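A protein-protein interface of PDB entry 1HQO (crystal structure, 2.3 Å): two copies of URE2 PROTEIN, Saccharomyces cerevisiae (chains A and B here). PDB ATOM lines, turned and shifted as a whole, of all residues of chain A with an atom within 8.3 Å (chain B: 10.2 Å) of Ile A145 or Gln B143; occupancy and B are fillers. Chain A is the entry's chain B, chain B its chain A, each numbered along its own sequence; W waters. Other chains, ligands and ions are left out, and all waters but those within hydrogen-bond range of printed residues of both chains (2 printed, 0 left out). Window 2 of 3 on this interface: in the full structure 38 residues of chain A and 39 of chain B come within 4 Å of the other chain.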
ATOM      1  N   ALA A 134     -33.396 -13.771  25.776  1.00  0.00           N
ATOM      2  CA  ALA A 134     -32.401 -14.805  25.627  1.00  0.00           C
ATOM      3  C   ALA A 134     -32.660 -15.515  24.304  1.00  0.00           C
ATOM      4  O   ALA A 134     -31.743 -15.746  23.530  1.00  0.00           O
ATOM      5  CB  ALA A 134     -32.512 -15.771  26.759  1.00  0.00           C
ATOM      6  N   HIS A 136     -34.340 -14.344  21.756  1.00  0.00           N
ATOM      7  CA  HIS A 136     -34.098 -13.411  20.661  1.00  0.00           C
ATOM      8  C   HIS A 136     -32.634 -13.401  20.298  1.00  0.00           C
ATOM      9  O   HIS A 136     -32.263 -13.700  19.165  1.00  0.00           O
ATOM     10  CB  HIS A 136     -34.498 -11.984  21.027  1.00  0.00           C
ATOM     11  CG  HIS A 136     -34.187 -10.986  19.951  1.00  0.00           C
ATOM     12  ND1 HIS A 136     -34.843 -10.970  18.736  1.00  0.00           N
ATOM     13  CD2 HIS A 136     -33.264  -9.997  19.893  1.00  0.00           C
ATOM     14  CE1 HIS A 136     -34.334 -10.014  17.979  1.00  0.00           C
ATOM     15  NE2 HIS A 136     -33.374  -9.410  18.658  1.00  0.00           N
ATOM     16  N   PHE A 137     -31.797 -13.067  21.270  1.00  0.00           N
ATOM     17  CA  PHE A 137     -30.371 -13.001  21.009  1.00  0.00           C
ATOM     18  C   PHE A 137     -29.655 -14.290  20.589  1.00  0.00           C
ATOM     19  O   PHE A 137     -28.588 -14.217  19.957  1.00  0.00           O
ATOM     20  CB  PHE A 137     -29.658 -12.341  22.191  1.00  0.00           C
ATOM     21  CG  PHE A 137     -29.817 -10.855  22.204  1.00  0.00           C
ATOM     22  CD1 PHE A 137     -30.689 -10.239  23.097  1.00  0.00           C
ATOM     23  CD2 PHE A 137     -29.172 -10.075  21.250  1.00  0.00           C
ATOM     24  CE1 PHE A 137     -30.927  -8.861  23.033  1.00  0.00           C
ATOM     25  CE2 PHE A 137     -29.399  -8.693  21.170  1.00  0.00           C
ATOM     26  CZ  PHE A 137     -30.278  -8.082  22.061  1.00  0.00           C
ATOM     27  N   ARG A 138     -30.228 -15.454  20.912  1.00  0.00           N
ATOM     28  CA  ARG A 138     -29.609 -16.732  20.542  1.00  0.00           C
ATOM     29  C   ARG A 138     -30.072 -17.200  19.198  1.00  0.00           C
ATOM     30  O   ARG A 138     -29.356 -17.909  18.503  1.00  0.00           O
ATOM     31  CB  ARG A 138     -29.936 -17.840  21.548  1.00  0.00           C
ATOM     32  CG  ARG A 138     -29.659 -19.244  21.018  1.00  0.00           C
ATOM     33  CD  ARG A 138     -29.006 -20.100  22.089  1.00  0.00           C
ATOM     34  NE  ARG A 138     -29.128 -21.540  21.827  1.00  0.00           N
ATOM     35  CZ  ARG A 138     -28.744 -22.506  22.677  1.00  0.00           C
ATOM     36  NH1 ARG A 138     -28.206 -22.194  23.860  1.00  0.00           N
ATOM     37  NH2 ARG A 138     -28.890 -23.791  22.345  1.00  0.00           N
ATOM     38  N   TYR A 139     -31.274 -16.791  18.835  1.00  0.00           N
ATOM     39  CA  TYR A 139     -31.858 -17.238  17.598  1.00  0.00           C
ATOM     40  C   TYR A 139     -32.257 -16.205  16.569  1.00  0.00           C
ATOM     41  O   TYR A 139     -32.131 -16.461  15.359  1.00  0.00           O
ATOM     42  CB  TYR A 139     -33.095 -18.073  17.903  1.00  0.00           C
ATOM     43  CG  TYR A 139     -32.815 -19.330  18.660  1.00  0.00           C
ATOM     44  CD1 TYR A 139     -33.306 -19.513  19.948  1.00  0.00           C
ATOM     45  CD2 TYR A 139     -32.087 -20.358  18.077  1.00  0.00           C
ATOM     46  CE1 TYR A 139     -33.081 -20.704  20.640  1.00  0.00           C
ATOM     47  CE2 TYR A 139     -31.853 -21.561  18.753  1.00  0.00           C
ATOM     48  CZ  TYR A 139     -32.354 -21.737  20.035  1.00  0.00           C
ATOM     49  OH  TYR A 139     -32.170 -22.951  20.677  1.00  0.00           O
ATOM     50  N   HIS A 141     -31.617 -12.347  16.717  1.00  0.00           N
ATOM     51  CA  HIS A 141     -30.965 -11.071  16.507  1.00  0.00           C
ATOM     52  C   HIS A 141     -30.112 -11.134  15.264  1.00  0.00           C
ATOM     53  O   HIS A 141     -29.440 -12.123  15.029  1.00  0.00           O
ATOM     54  CB  HIS A 141     -30.091 -10.707  17.691  1.00  0.00           C
ATOM     55  CG  HIS A 141     -29.832  -9.237  17.814  1.00  0.00           C
ATOM     56  ND1 HIS A 141     -30.849  -8.313  17.931  1.00  0.00           N
ATOM     57  CD2 HIS A 141     -28.674  -8.534  17.879  1.00  0.00           C
ATOM     58  CE1 HIS A 141     -30.330  -7.106  18.066  1.00  0.00           C
ATOM     59  NE2 HIS A 141     -29.011  -7.213  18.038  1.00  0.00           N
ATOM     60  N   SER A 142     -30.144 -10.072  14.476  1.00  0.00           N
ATOM     61  CA  SER A 142     -29.356  -9.999  13.255  1.00  0.00           C
ATOM     62  C   SER A 142     -27.902 -10.374  13.493  1.00  0.00           C
ATOM     63  O   SER A 142     -27.275 -11.011  12.654  1.00  0.00           O
ATOM     64  CB  SER A 142     -29.417  -8.582  12.713  1.00  0.00           C
ATOM     65  OG  SER A 142     -29.185  -7.663  13.770  1.00  0.00           O
ATOM     66  N   GLN A 143     -27.375  -9.960  14.643  1.00  0.00           N
ATOM     67  CA  GLN A 143     -25.988 -10.223  15.031  1.00  0.00           C
ATOM     68  C   GLN A 143     -26.033 -11.166  16.252  1.00  0.00           C
ATOM     69  O   GLN A 143     -26.661 -10.843  17.259  1.00  0.00           O
ATOM     70  CB  GLN A 143     -25.301  -8.871  15.374  1.00  0.00           C
ATOM     71  CG  GLN A 143     -23.741  -8.847  15.376  1.00  0.00           C
ATOM     72  CD  GLN A 143     -23.098  -9.151  13.995  1.00  0.00           C
ATOM     73  OE1 GLN A 143     -23.327  -8.433  13.005  1.00  0.00           O
ATOM     74  NE2 GLN A 143     -22.285 -10.219  13.937  1.00  0.00           N
ATOM     75  N   LYS A 144     -25.379 -12.326  16.157  1.00  0.00           N
ATOM     76  CA  LYS A 144     -25.359 -13.316  17.246  1.00  0.00           C
ATOM     77  C   LYS A 144     -24.306 -13.011  18.313  1.00  0.00           C
ATOM     78  O   LYS A 144     -23.258 -13.663  18.372  1.00  0.00           O
ATOM     79  CB  LYS A 144     -25.110 -14.712  16.670  1.00  0.00           C
ATOM     80  CG  LYS A 144     -25.385 -15.863  17.637  1.00  0.00           C
ATOM     81  CD  LYS A 144     -25.329 -17.219  16.917  1.00  0.00           C
ATOM     82  CE  LYS A 144     -25.734 -18.358  17.829  1.00  0.00           C
ATOM     83  NZ  LYS A 144     -25.997 -19.562  17.005  1.00  0.00           N
ATOM     84  N   ILE A 145     -24.619 -12.045  19.177  1.00  0.00           N
ATOM     85  CA  ILE A 145     -23.712 -11.585  20.230  1.00  0.00           C
ATOM     86  C   ILE A 145     -23.699 -12.352  21.557  1.00  0.00           C
ATOM     87  O   ILE A 145     -24.618 -12.233  22.372  1.00  0.00           O
ATOM     88  CB  ILE A 145     -23.986 -10.109  20.523  1.00  0.00           C
ATOM     89  CG1 ILE A 145     -24.008  -9.347  19.197  1.00  0.00           C
ATOM     90  CG2 ILE A 145     -22.929  -9.555  21.473  1.00  0.00           C
ATOM     91  CD1 ILE A 145     -24.482  -7.931  19.304  1.00  0.00           C
ATOM     92  N   ALA A 146     -22.625 -13.105  21.779  1.00  0.00           N
ATOM     93  CA  ALA A 146     -22.474 -13.902  22.984  1.00  0.00           C
ATOM     94  C   ALA A 146     -22.730 -13.196  24.308  1.00  0.00           C
ATOM     95  O   ALA A 146     -23.457 -13.740  25.131  1.00  0.00           O
ATOM     96  CB  ALA A 146     -21.113 -14.532  23.012  1.00  0.00           C
ATOM     97  N   SER A 147     -22.140 -12.018  24.533  1.00  0.00           N
ATOM     98  CA  SER A 147     -22.334 -11.283  25.797  1.00  0.00           C
ATOM     99  C   SER A 147     -23.794 -10.970  26.095  1.00  0.00           C
ATOM    100  O   SER A 147     -24.202 -10.894  27.264  1.00  0.00           O
ATOM    101  CB  SER A 147     -21.562  -9.972  25.772  1.00  0.00           C
ATOM    102  OG  SER A 147     -21.959  -9.180  24.667  1.00  0.00           O
ATOM    103  N   ALA A 148     -24.562 -10.768  25.020  1.00  0.00           N
ATOM    104  CA  ALA A 148     -25.987 -10.466  25.102  1.00  0.00           C
ATOM    105  C   ALA A 148     -26.699 -11.700  25.628  1.00  0.00           C
ATOM    106  O   ALA A 148     -27.448 -11.648  26.609  1.00  0.00           O
ATOM    107  CB  ALA A 148     -26.523 -10.102  23.729  1.00  0.00           C
ATOM    108  N   VAL A 149     -26.440 -12.819  24.971  1.00  0.00           N
ATOM    109  CA  VAL A 149     -27.035 -14.082  25.345  1.00  0.00           C
ATOM    110  C   VAL A 149     -26.761 -14.513  26.783  1.00  0.00           C
ATOM    111  O   VAL A 149     -27.646 -15.011  27.468  1.00  0.00           O
ATOM    112  CB  VAL A 149     -26.541 -15.159  24.415  1.00  0.00           C
ATOM    113  CG1 VAL A 149     -27.192 -16.478  24.764  1.00  0.00           C
ATOM    114  CG2 VAL A 149     -26.830 -14.761  22.990  1.00  0.00           C
ATOM    115  N   GLU A 150     -25.534 -14.331  27.241  1.00  0.00           N
ATOM    116  CA  GLU A 150     -25.175 -14.737  28.588  1.00  0.00           C
ATOM    117  C   GLU A 150     -25.937 -13.894  29.566  1.00  0.00           C
ATOM    118  O   GLU A 150     -26.374 -14.389  30.599  1.00  0.00           O
ATOM    119  CB  GLU A 150     -23.685 -14.542  28.836  1.00  0.00           C
ATOM    120  CG  GLU A 150     -22.777 -14.897  27.658  1.00  0.00           C
ATOM    121  CD  GLU A 150     -22.789 -16.380  27.285  1.00  0.00           C
ATOM    122  OE1 GLU A 150     -23.733 -16.859  26.608  1.00  0.00           O
ATOM    123  OE2 GLU A 150     -21.826 -17.071  27.680  1.00  0.00           O
ATOM    124  N   ARG A 151     -26.091 -12.612  29.232  1.00  0.00           N
ATOM    125  CA  ARG A 151     -26.804 -11.663  30.093  1.00  0.00           C
ATOM    126  C   ARG A 151     -28.149 -12.226  30.497  1.00  0.00           C
ATOM    127  O   ARG A 151     -28.495 -12.303  31.676  1.00  0.00           O
ATOM    128  CB  ARG A 151     -27.017 -10.314  29.374  1.00  0.00           C
ATOM    129  CG  ARG A 151     -27.803  -9.307  30.219  1.00  0.00           C
ATOM    130  CD  ARG A 151     -28.010  -7.952  29.554  1.00  0.00           C
ATOM    131  NE  ARG A 151     -29.110  -7.213  30.188  1.00  0.00           N
ATOM    132  CZ  ARG A 151     -29.158  -6.869  31.476  1.00  0.00           C
ATOM    133  NH1 ARG A 151     -28.158  -7.190  32.293  1.00  0.00           N
ATOM    134  NH2 ARG A 151     -30.221  -6.221  31.950  1.00  0.00           N
ATOM    135  N   TYR A 152     -28.886 -12.644  29.485  1.00  0.00           N
ATOM    136  CA  TYR A 152     -30.206 -13.161  29.678  1.00  0.00           C
ATOM    137  C   TYR A 152     -30.239 -14.582  30.145  1.00  0.00           C
ATOM    138  O   TYR A 152     -31.120 -14.957  30.919  1.00  0.00           O
ATOM    139  CB  TYR A 152     -30.988 -12.974  28.394  1.00  0.00           C
ATOM    140  CG  TYR A 152     -31.165 -11.506  28.112  1.00  0.00           C
ATOM    141  CD1 TYR A 152     -30.550 -10.889  27.017  1.00  0.00           C
ATOM    142  CD2 TYR A 152     -31.878 -10.704  29.002  1.00  0.00           C
ATOM    143  CE1 TYR A 152     -30.633  -9.493  26.818  1.00  0.00           C
ATOM    144  CE2 TYR A 152     -31.973  -9.317  28.825  1.00  0.00           C
ATOM    145  CZ  TYR A 152     -31.345  -8.716  27.733  1.00  0.00           C
ATOM    146  OH  TYR A 152     -31.411  -7.332  27.606  1.00  0.00           O
ATOM    147  N   LEU B 135     -31.687   1.022  28.930  1.00  0.00           N
ATOM    148  CA  LEU B 135     -30.705   1.748  29.728  1.00  0.00           C
ATOM    149  C   LEU B 135     -29.472   0.886  29.887  1.00  0.00           C
ATOM    150  O   LEU B 135     -28.359   1.386  29.889  1.00  0.00           O
ATOM    151  CB  LEU B 135     -31.229   2.109  31.119  1.00  0.00           C
ATOM    152  CG  LEU B 135     -30.189   2.907  31.925  1.00  0.00           C
ATOM    153  CD1 LEU B 135     -30.131   4.339  31.452  1.00  0.00           C
ATOM    154  CD2 LEU B 135     -30.540   2.877  33.402  1.00  0.00           C
ATOM    155  N   HIS B 136     -29.665  -0.419  30.011  1.00  0.00           N
ATOM    156  CA  HIS B 136     -28.534  -1.322  30.172  1.00  0.00           C
ATOM    157  C   HIS B 136     -27.606  -1.237  28.991  1.00  0.00           C
ATOM    158  O   HIS B 136     -26.474  -0.800  29.125  1.00  0.00           O
ATOM    159  CB  HIS B 136     -28.967  -2.780  30.304  1.00  0.00           C
ATOM    160  CG  HIS B 136     -27.822  -3.746  30.290  1.00  0.00           C
ATOM    161  ND1 HIS B 136     -26.980  -3.925  31.367  1.00  0.00           N
ATOM    162  CD2 HIS B 136     -27.346  -4.544  29.306  1.00  0.00           C
ATOM    163  CE1 HIS B 136     -26.035  -4.789  31.047  1.00  0.00           C
ATOM    164  NE2 HIS B 136     -26.233  -5.179  29.801  1.00  0.00           N
ATOM    165  N   PHE B 137     -28.071  -1.677  27.830  1.00  0.00           N
ATOM    166  CA  PHE B 137     -27.221  -1.637  26.649  1.00  0.00           C
ATOM    167  C   PHE B 137     -26.649  -0.242  26.326  1.00  0.00           C
ATOM    168  O   PHE B 137     -25.693  -0.115  25.547  1.00  0.00           O
ATOM    169  CB  PHE B 137     -27.964  -2.203  25.436  1.00  0.00           C
ATOM    170  CG  PHE B 137     -28.100  -3.685  25.468  1.00  0.00           C
ATOM    171  CD1 PHE B 137     -29.268  -4.283  25.897  1.00  0.00           C
ATOM    172  CD2 PHE B 137     -27.032  -4.490  25.132  1.00  0.00           C
ATOM    173  CE1 PHE B 137     -29.361  -5.675  25.997  1.00  0.00           C
ATOM    174  CE2 PHE B 137     -27.110  -5.876  25.228  1.00  0.00           C
ATOM    175  CZ  PHE B 137     -28.278  -6.469  25.662  1.00  0.00           C
ATOM    176  N   ARG B 138     -27.223   0.792  26.931  1.00  0.00           N
ATOM    177  CA  ARG B 138     -26.754   2.150  26.727  1.00  0.00           C
ATOM    178  C   ARG B 138     -25.552   2.468  27.614  1.00  0.00           C
ATOM    179  O   ARG B 138     -24.503   2.901  27.132  1.00  0.00           O
ATOM    180  CB  ARG B 138     -27.877   3.146  27.021  1.00  0.00           C
ATOM    181  CG  ARG B 138     -28.643   3.544  25.803  1.00  0.00           C
ATOM    182  CD  ARG B 138     -28.094   4.833  25.248  1.00  0.00           C
ATOM    183  NE  ARG B 138     -28.923   5.962  25.647  1.00  0.00           N
ATOM    184  CZ  ARG B 138     -28.641   7.221  25.348  1.00  0.00           C
ATOM    185  NH1 ARG B 138     -27.542   7.490  24.652  1.00  0.00           N
ATOM    186  NH2 ARG B 138     -29.455   8.203  25.727  1.00  0.00           N
ATOM    187  N   TYR B 139     -25.680   2.225  28.910  1.00  0.00           N
ATOM    188  CA  TYR B 139     -24.581   2.566  29.776  1.00  0.00           C
ATOM    189  C   TYR B 139     -23.932   1.477  30.627  1.00  0.00           C
ATOM    190  O   TYR B 139     -23.022   1.777  31.393  1.00  0.00           O
ATOM    191  CB  TYR B 139     -25.018   3.699  30.689  1.00  0.00           C
ATOM    192  CG  TYR B 139     -25.761   4.832  30.011  1.00  0.00           C
ATOM    193  CD1 TYR B 139     -27.148   4.882  30.038  1.00  0.00           C
ATOM    194  CD2 TYR B 139     -25.074   5.898  29.412  1.00  0.00           C
ATOM    195  CE1 TYR B 139     -27.839   5.968  29.501  1.00  0.00           C
ATOM    196  CE2 TYR B 139     -25.761   6.989  28.868  1.00  0.00           C
ATOM    197  CZ  TYR B 139     -27.145   7.018  28.924  1.00  0.00           C
ATOM    198  OH  TYR B 139     -27.853   8.104  28.458  1.00  0.00           O
ATOM    199  N   PHE B 140     -24.337   0.221  30.506  1.00  0.00           N
ATOM    200  CA  PHE B 140     -23.741  -0.771  31.389  1.00  0.00           C
ATOM    201  C   PHE B 140     -23.321  -2.077  30.771  1.00  0.00           C
ATOM    202  O   PHE B 140     -22.842  -2.970  31.465  1.00  0.00           O
ATOM    203  CB  PHE B 140     -24.692  -1.128  32.531  1.00  0.00           C
ATOM    204  CG  PHE B 140     -25.177   0.045  33.336  1.00  0.00           C
ATOM    205  CD1 PHE B 140     -26.247   0.828  32.897  1.00  0.00           C
ATOM    206  CD2 PHE B 140     -24.600   0.330  34.578  1.00  0.00           C
ATOM    207  CE1 PHE B 140     -26.739   1.872  33.690  1.00  0.00           C
ATOM    208  CE2 PHE B 140     -25.087   1.375  35.385  1.00  0.00           C
ATOM    209  CZ  PHE B 140     -26.159   2.144  34.938  1.00  0.00           C
ATOM    210  N   HIS B 141     -23.502  -2.243  29.482  1.00  0.00           N
ATOM    211  CA  HIS B 141     -23.109  -3.524  28.936  1.00  0.00           C
ATOM    212  C   HIS B 141     -21.600  -3.592  28.832  1.00  0.00           C
ATOM    213  O   HIS B 141     -20.928  -2.560  28.862  1.00  0.00           O
ATOM    214  CB  HIS B 141     -23.733  -3.726  27.559  1.00  0.00           C
ATOM    215  CG  HIS B 141     -23.721  -5.151  27.105  1.00  0.00           C
ATOM    216  ND1 HIS B 141     -24.152  -6.194  27.915  1.00  0.00           N
ATOM    217  CD2 HIS B 141     -23.431  -5.699  25.896  1.00  0.00           C
ATOM    218  CE1 HIS B 141     -24.140  -7.321  27.219  1.00  0.00           C
ATOM    219  NE2 HIS B 141     -23.710  -7.047  25.990  1.00  0.00           N
ATOM    220  N   SER B 142     -21.075  -4.804  28.721  1.00  0.00           N
ATOM    221  CA  SER B 142     -19.641  -4.994  28.589  1.00  0.00           C
ATOM    222  C   SER B 142     -19.256  -4.493  27.203  1.00  0.00           C
ATOM    223  O   SER B 142     -18.368  -3.650  27.049  1.00  0.00           O
ATOM    224  CB  SER B 142     -19.289  -6.474  28.717  1.00  0.00           C
ATOM    225  OG  SER B 142     -19.906  -7.236  27.693  1.00  0.00           O
ATOM    226  N   GLN B 143     -19.947  -5.011  26.193  1.00  0.00           N
ATOM    227  CA  GLN B 143     -19.701  -4.633  24.809  1.00  0.00           C
ATOM    228  C   GLN B 143     -20.495  -3.391  24.437  1.00  0.00           C
ATOM    229  O   GLN B 143     -20.986  -2.682  25.299  1.00  0.00           O
ATOM    230  CB  GLN B 143     -20.133  -5.762  23.913  1.00  0.00           C
ATOM    231  CG  GLN B 143     -19.068  -6.273  23.038  1.00  0.00           C
ATOM    232  CD  GLN B 143     -19.472  -7.604  22.498  1.00  0.00           C
ATOM    233  OE1 GLN B 143     -19.761  -8.525  23.268  1.00  0.00           O
ATOM    234  NE2 GLN B 143     -19.521  -7.727  21.174  1.00  0.00           N
ATOM    235  N   LYS B 144     -20.631  -3.130  23.147  1.00  0.00           N
ATOM    236  CA  LYS B 144     -21.389  -1.975  22.710  1.00  0.00           C
ATOM    237  C   LYS B 144     -22.062  -2.337  21.414  1.00  0.00           C
ATOM    238  O   LYS B 144     -21.456  -2.315  20.345  1.00  0.00           O
ATOM    239  CB  LYS B 144     -20.481  -0.788  22.492  1.00  0.00           C
ATOM    240  CG  LYS B 144     -21.243   0.502  22.279  1.00  0.00           C
ATOM    241  CD  LYS B 144     -21.811   1.052  23.593  1.00  0.00           C
ATOM    242  CE  LYS B 144     -22.484   2.413  23.361  1.00  0.00           C
ATOM    243  NZ  LYS B 144     -23.030   3.028  24.605  1.00  0.00           N
ATOM    244  N   ILE B 145     -23.330  -2.672  21.520  1.00  0.00           N
ATOM    245  CA  ILE B 145     -24.094  -3.085  20.371  1.00  0.00           C
ATOM    246  C   ILE B 145     -25.114  -2.012  20.069  1.00  0.00           C
ATOM    247  O   ILE B 145     -26.064  -1.821  20.815  1.00  0.00           O
ATOM    248  CB  ILE B 145     -24.788  -4.397  20.687  1.00  0.00           C
ATOM    249  CG1 ILE B 145     -23.787  -5.329  21.368  1.00  0.00           C
ATOM    250  CG2 ILE B 145     -25.343  -5.007  19.428  1.00  0.00           C
ATOM    251  CD1 ILE B 145     -24.346  -6.117  22.540  1.00  0.00           C
ATOM    252  N   ALA B 146     -24.912  -1.292  18.981  1.00  0.00           N
ATOM    253  CA  ALA B 146     -25.834  -0.234  18.635  1.00  0.00           C
ATOM    254  C   ALA B 146     -27.164  -0.871  18.340  1.00  0.00           C
ATOM    255  O   ALA B 146     -28.228  -0.294  18.558  1.00  0.00           O
ATOM    256  CB  ALA B 146     -25.337   0.483  17.431  1.00  0.00           C
ATOM    257  N   SER B 147     -27.091  -2.087  17.839  1.00  0.00           N
ATOM    258  CA  SER B 147     -28.296  -2.802  17.503  1.00  0.00           C
ATOM    259  C   SER B 147     -29.102  -3.216  18.735  1.00  0.00           C
ATOM    260  O   SER B 147     -30.327  -3.264  18.683  1.00  0.00           O
ATOM    261  CB  SER B 147     -27.971  -4.029  16.632  1.00  0.00           C
ATOM    262  OG  SER B 147     -27.196  -5.002  17.311  1.00  0.00           O
ATOM    263  N   ALA B 148     -28.428  -3.522  19.838  1.00  0.00           N
ATOM    264  CA  ALA B 148     -29.128  -3.911  21.053  1.00  0.00           C
ATOM    265  C   ALA B 148     -29.907  -2.710  21.574  1.00  0.00           C
ATOM    266  O   ALA B 148     -31.057  -2.852  21.950  1.00  0.00           O
ATOM    267  CB  ALA B 148     -28.144  -4.401  22.101  1.00  0.00           C
ATOM    268  N   VAL B 149     -29.274  -1.533  21.574  1.00  0.00           N
ATOM    269  CA  VAL B 149     -29.888  -0.286  22.042  1.00  0.00           C
ATOM    270  C   VAL B 149     -31.071   0.117  21.181  1.00  0.00           C
ATOM    271  O   VAL B 149     -32.110   0.530  21.687  1.00  0.00           O
ATOM    272  CB  VAL B 149     -28.883   0.884  22.035  1.00  0.00           C
ATOM    273  CG1 VAL B 149     -29.612   2.191  22.370  1.00  0.00           C
ATOM    274  CG2 VAL B 149     -27.758   0.612  23.037  1.00  0.00           C
ATOM    275  N   ARG B 151     -32.870  -1.833  19.338  1.00  0.00           N
ATOM    276  CA  ARG B 151     -33.900  -2.829  19.566  1.00  0.00           C
ATOM    277  C   ARG B 151     -34.863  -2.392  20.653  1.00  0.00           C
ATOM    278  O   ARG B 151     -36.076  -2.438  20.461  1.00  0.00           O
ATOM    279  CB  ARG B 151     -33.279  -4.158  19.973  1.00  0.00           C
ATOM    280  CG  ARG B 151     -34.307  -5.149  20.437  1.00  0.00           C
ATOM    281  CD  ARG B 151     -33.653  -6.458  20.804  1.00  0.00           C
ATOM    282  NE  ARG B 151     -34.578  -7.375  21.471  1.00  0.00           N
ATOM    283  CZ  ARG B 151     -35.662  -7.905  20.909  1.00  0.00           C
ATOM    284  NH1 ARG B 151     -35.986  -7.629  19.650  1.00  0.00           N
ATOM    285  NH2 ARG B 151     -36.446  -8.696  21.619  1.00  0.00           N
ATOM    286  N   TYR B 152     -34.308  -1.964  21.786  1.00  0.00           N
ATOM    287  CA  TYR B 152     -35.083  -1.530  22.929  1.00  0.00           C
ATOM    288  C   TYR B 152     -35.645  -0.119  22.892  1.00  0.00           C
ATOM    289  O   TYR B 152     -36.745   0.092  23.414  1.00  0.00           O
ATOM    290  CB  TYR B 152     -34.264  -1.750  24.182  1.00  0.00           C
ATOM    291  CG  TYR B 152     -34.004  -3.215  24.390  1.00  0.00           C
ATOM    292  CD1 TYR B 152     -32.718  -3.740  24.326  1.00  0.00           C
ATOM    293  CD2 TYR B 152     -35.066  -4.094  24.592  1.00  0.00           C
ATOM    294  CE1 TYR B 152     -32.499  -5.115  24.451  1.00  0.00           C
ATOM    295  CE2 TYR B 152     -34.861  -5.460  24.719  1.00  0.00           C
ATOM    296  CZ  TYR B 152     -33.581  -5.970  24.640  1.00  0.00           C
ATOM    297  OH  TYR B 152     -33.411  -7.336  24.667  1.00  0.00           O
HETATM  298  O   HOH W   1     -19.645 -11.167  22.822  1.00  0.00           O
HETATM  299  O   HOH W   2     -24.958  -8.080  31.237  1.00  0.00           O
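A ring nitrogen (NE2) of His B141 lies within hydrogen-bond range of the side-chain hydroxyl of Ser A147, at 3.1 Å.
The side-chain amide oxygen of Gln B143 is in hydrogen-bond range of the side-chain hydroxyl of Ser A147, 2.7 Å away.
A ring nitrogen (NE2) of His A141 sits at hydrogen-bond distance from the side-chain hydroxyl (OG) of Ser B147, 3.0 Å away.
The guanidinium group of Arg B151 lies within hydrogen-bond range of a ring nitrogen (NE2) of His A136 (3.3 Å).
NE2 of His B136 is in hydrogen-bond range of ND1 of His B141.
The guanidinium group (NE) of Arg B151 lies within hydrogen-bond range of the side-chain hydroxyl (OH) of Tyr B152 (3.4 Å).
A ring nitrogen (NE2) of His A136 lies within hydrogen-bond range of a ring nitrogen (ND1) of His A141 (2.8 Å).
NE of Arg A151 lies within hydrogen-bond range of OH of Tyr A152 (3.5 Å).
Among the printed residues, merely in contact across the chains: Ile A145 with Ile B145 (3.1 Å), Tyr A152 with Phe B137 (3.1 Å), Arg A151 with His B136 (3.3 Å), Phe A137 with Tyr B152 (3.3 Å), Tyr A152 with Tyr B152 (3.6 Å), Ser A147 with Ser B142 (3.7 Å), Ile A145 with Gln B143 (3.8 Å), Ala A148 with His B141 (3.9 Å) and Phe A137 with Arg B151 (3.95 Å).
Of chain B, only Gln B143 (3.8 Å) and Ile B145 (3.1 Å) come within 4 Å of Ile A145.
Gln B143 touches just these residues of chain A: Ile A145 (3.8 Å) and Ser A147 (2.7 Å).
No residue of chain B comes within 4 Å of Ala A146.
Of chain B, only His B141 (3.9 Å) comes within 4 Å of Ala A148.
Ser B142 touches just one residue of chain A: Ser A147 (3.7 Å).
Of the printed residues of chain B, Phe A137 touches Arg B151 and Tyr B152.
Of the printed residues of chain A, Arg B151 touches His A136 and Phe A137.
Ala B146 touches none of the printed residues of chain A.
The nearest printed residue of chain A that does not touch Gln B143 is Ala A148 (5.6 Å).
Printed residues of chain A that touch a printed residue of chain B: His A136, Phe A137, His A141, Ile A145, Ser A147, Ala A148, Arg A151 and Tyr A152.
Hydrophobic or aromatic side chains of chain A that line the printed part of chain B: His A136, Phe A137, His A141, Ile A145 and Tyr A152.
Among the printed residues, 13 pairs touch across the chains.
Among the printed residues, no Asp or Glu carboxylate lies within 4 Å of a Lys or Arg side-chain nitrogen of the other chain.
His A136 touches Arg B151, and with the chains exchanged Arg A151 touches His B136.
Ser A147 touches Ser B142, but with the chains exchanged Ser A142 does not touch Ser B147 (4.8 Å).
Ser A147 touches Gln B143, but with the chains exchanged Gln A143 does not touch Ser B147 (4.7 Å).
Ala A148 touches His B141, but with the chains exchanged His A141 does not touch Ala B148 (4.1 Å).
15 positions are printed for both chains.
Water W1 lies within hydrogen-bond range of the side-chain amide oxygen (OE1) of Gln B143 (2.7 Å) and the backbone NH (N) of Ser A147 (3.1 Å).
Water W2 lies within hydrogen-bond range of NE2 of His B136 and NH1 of Arg A151.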
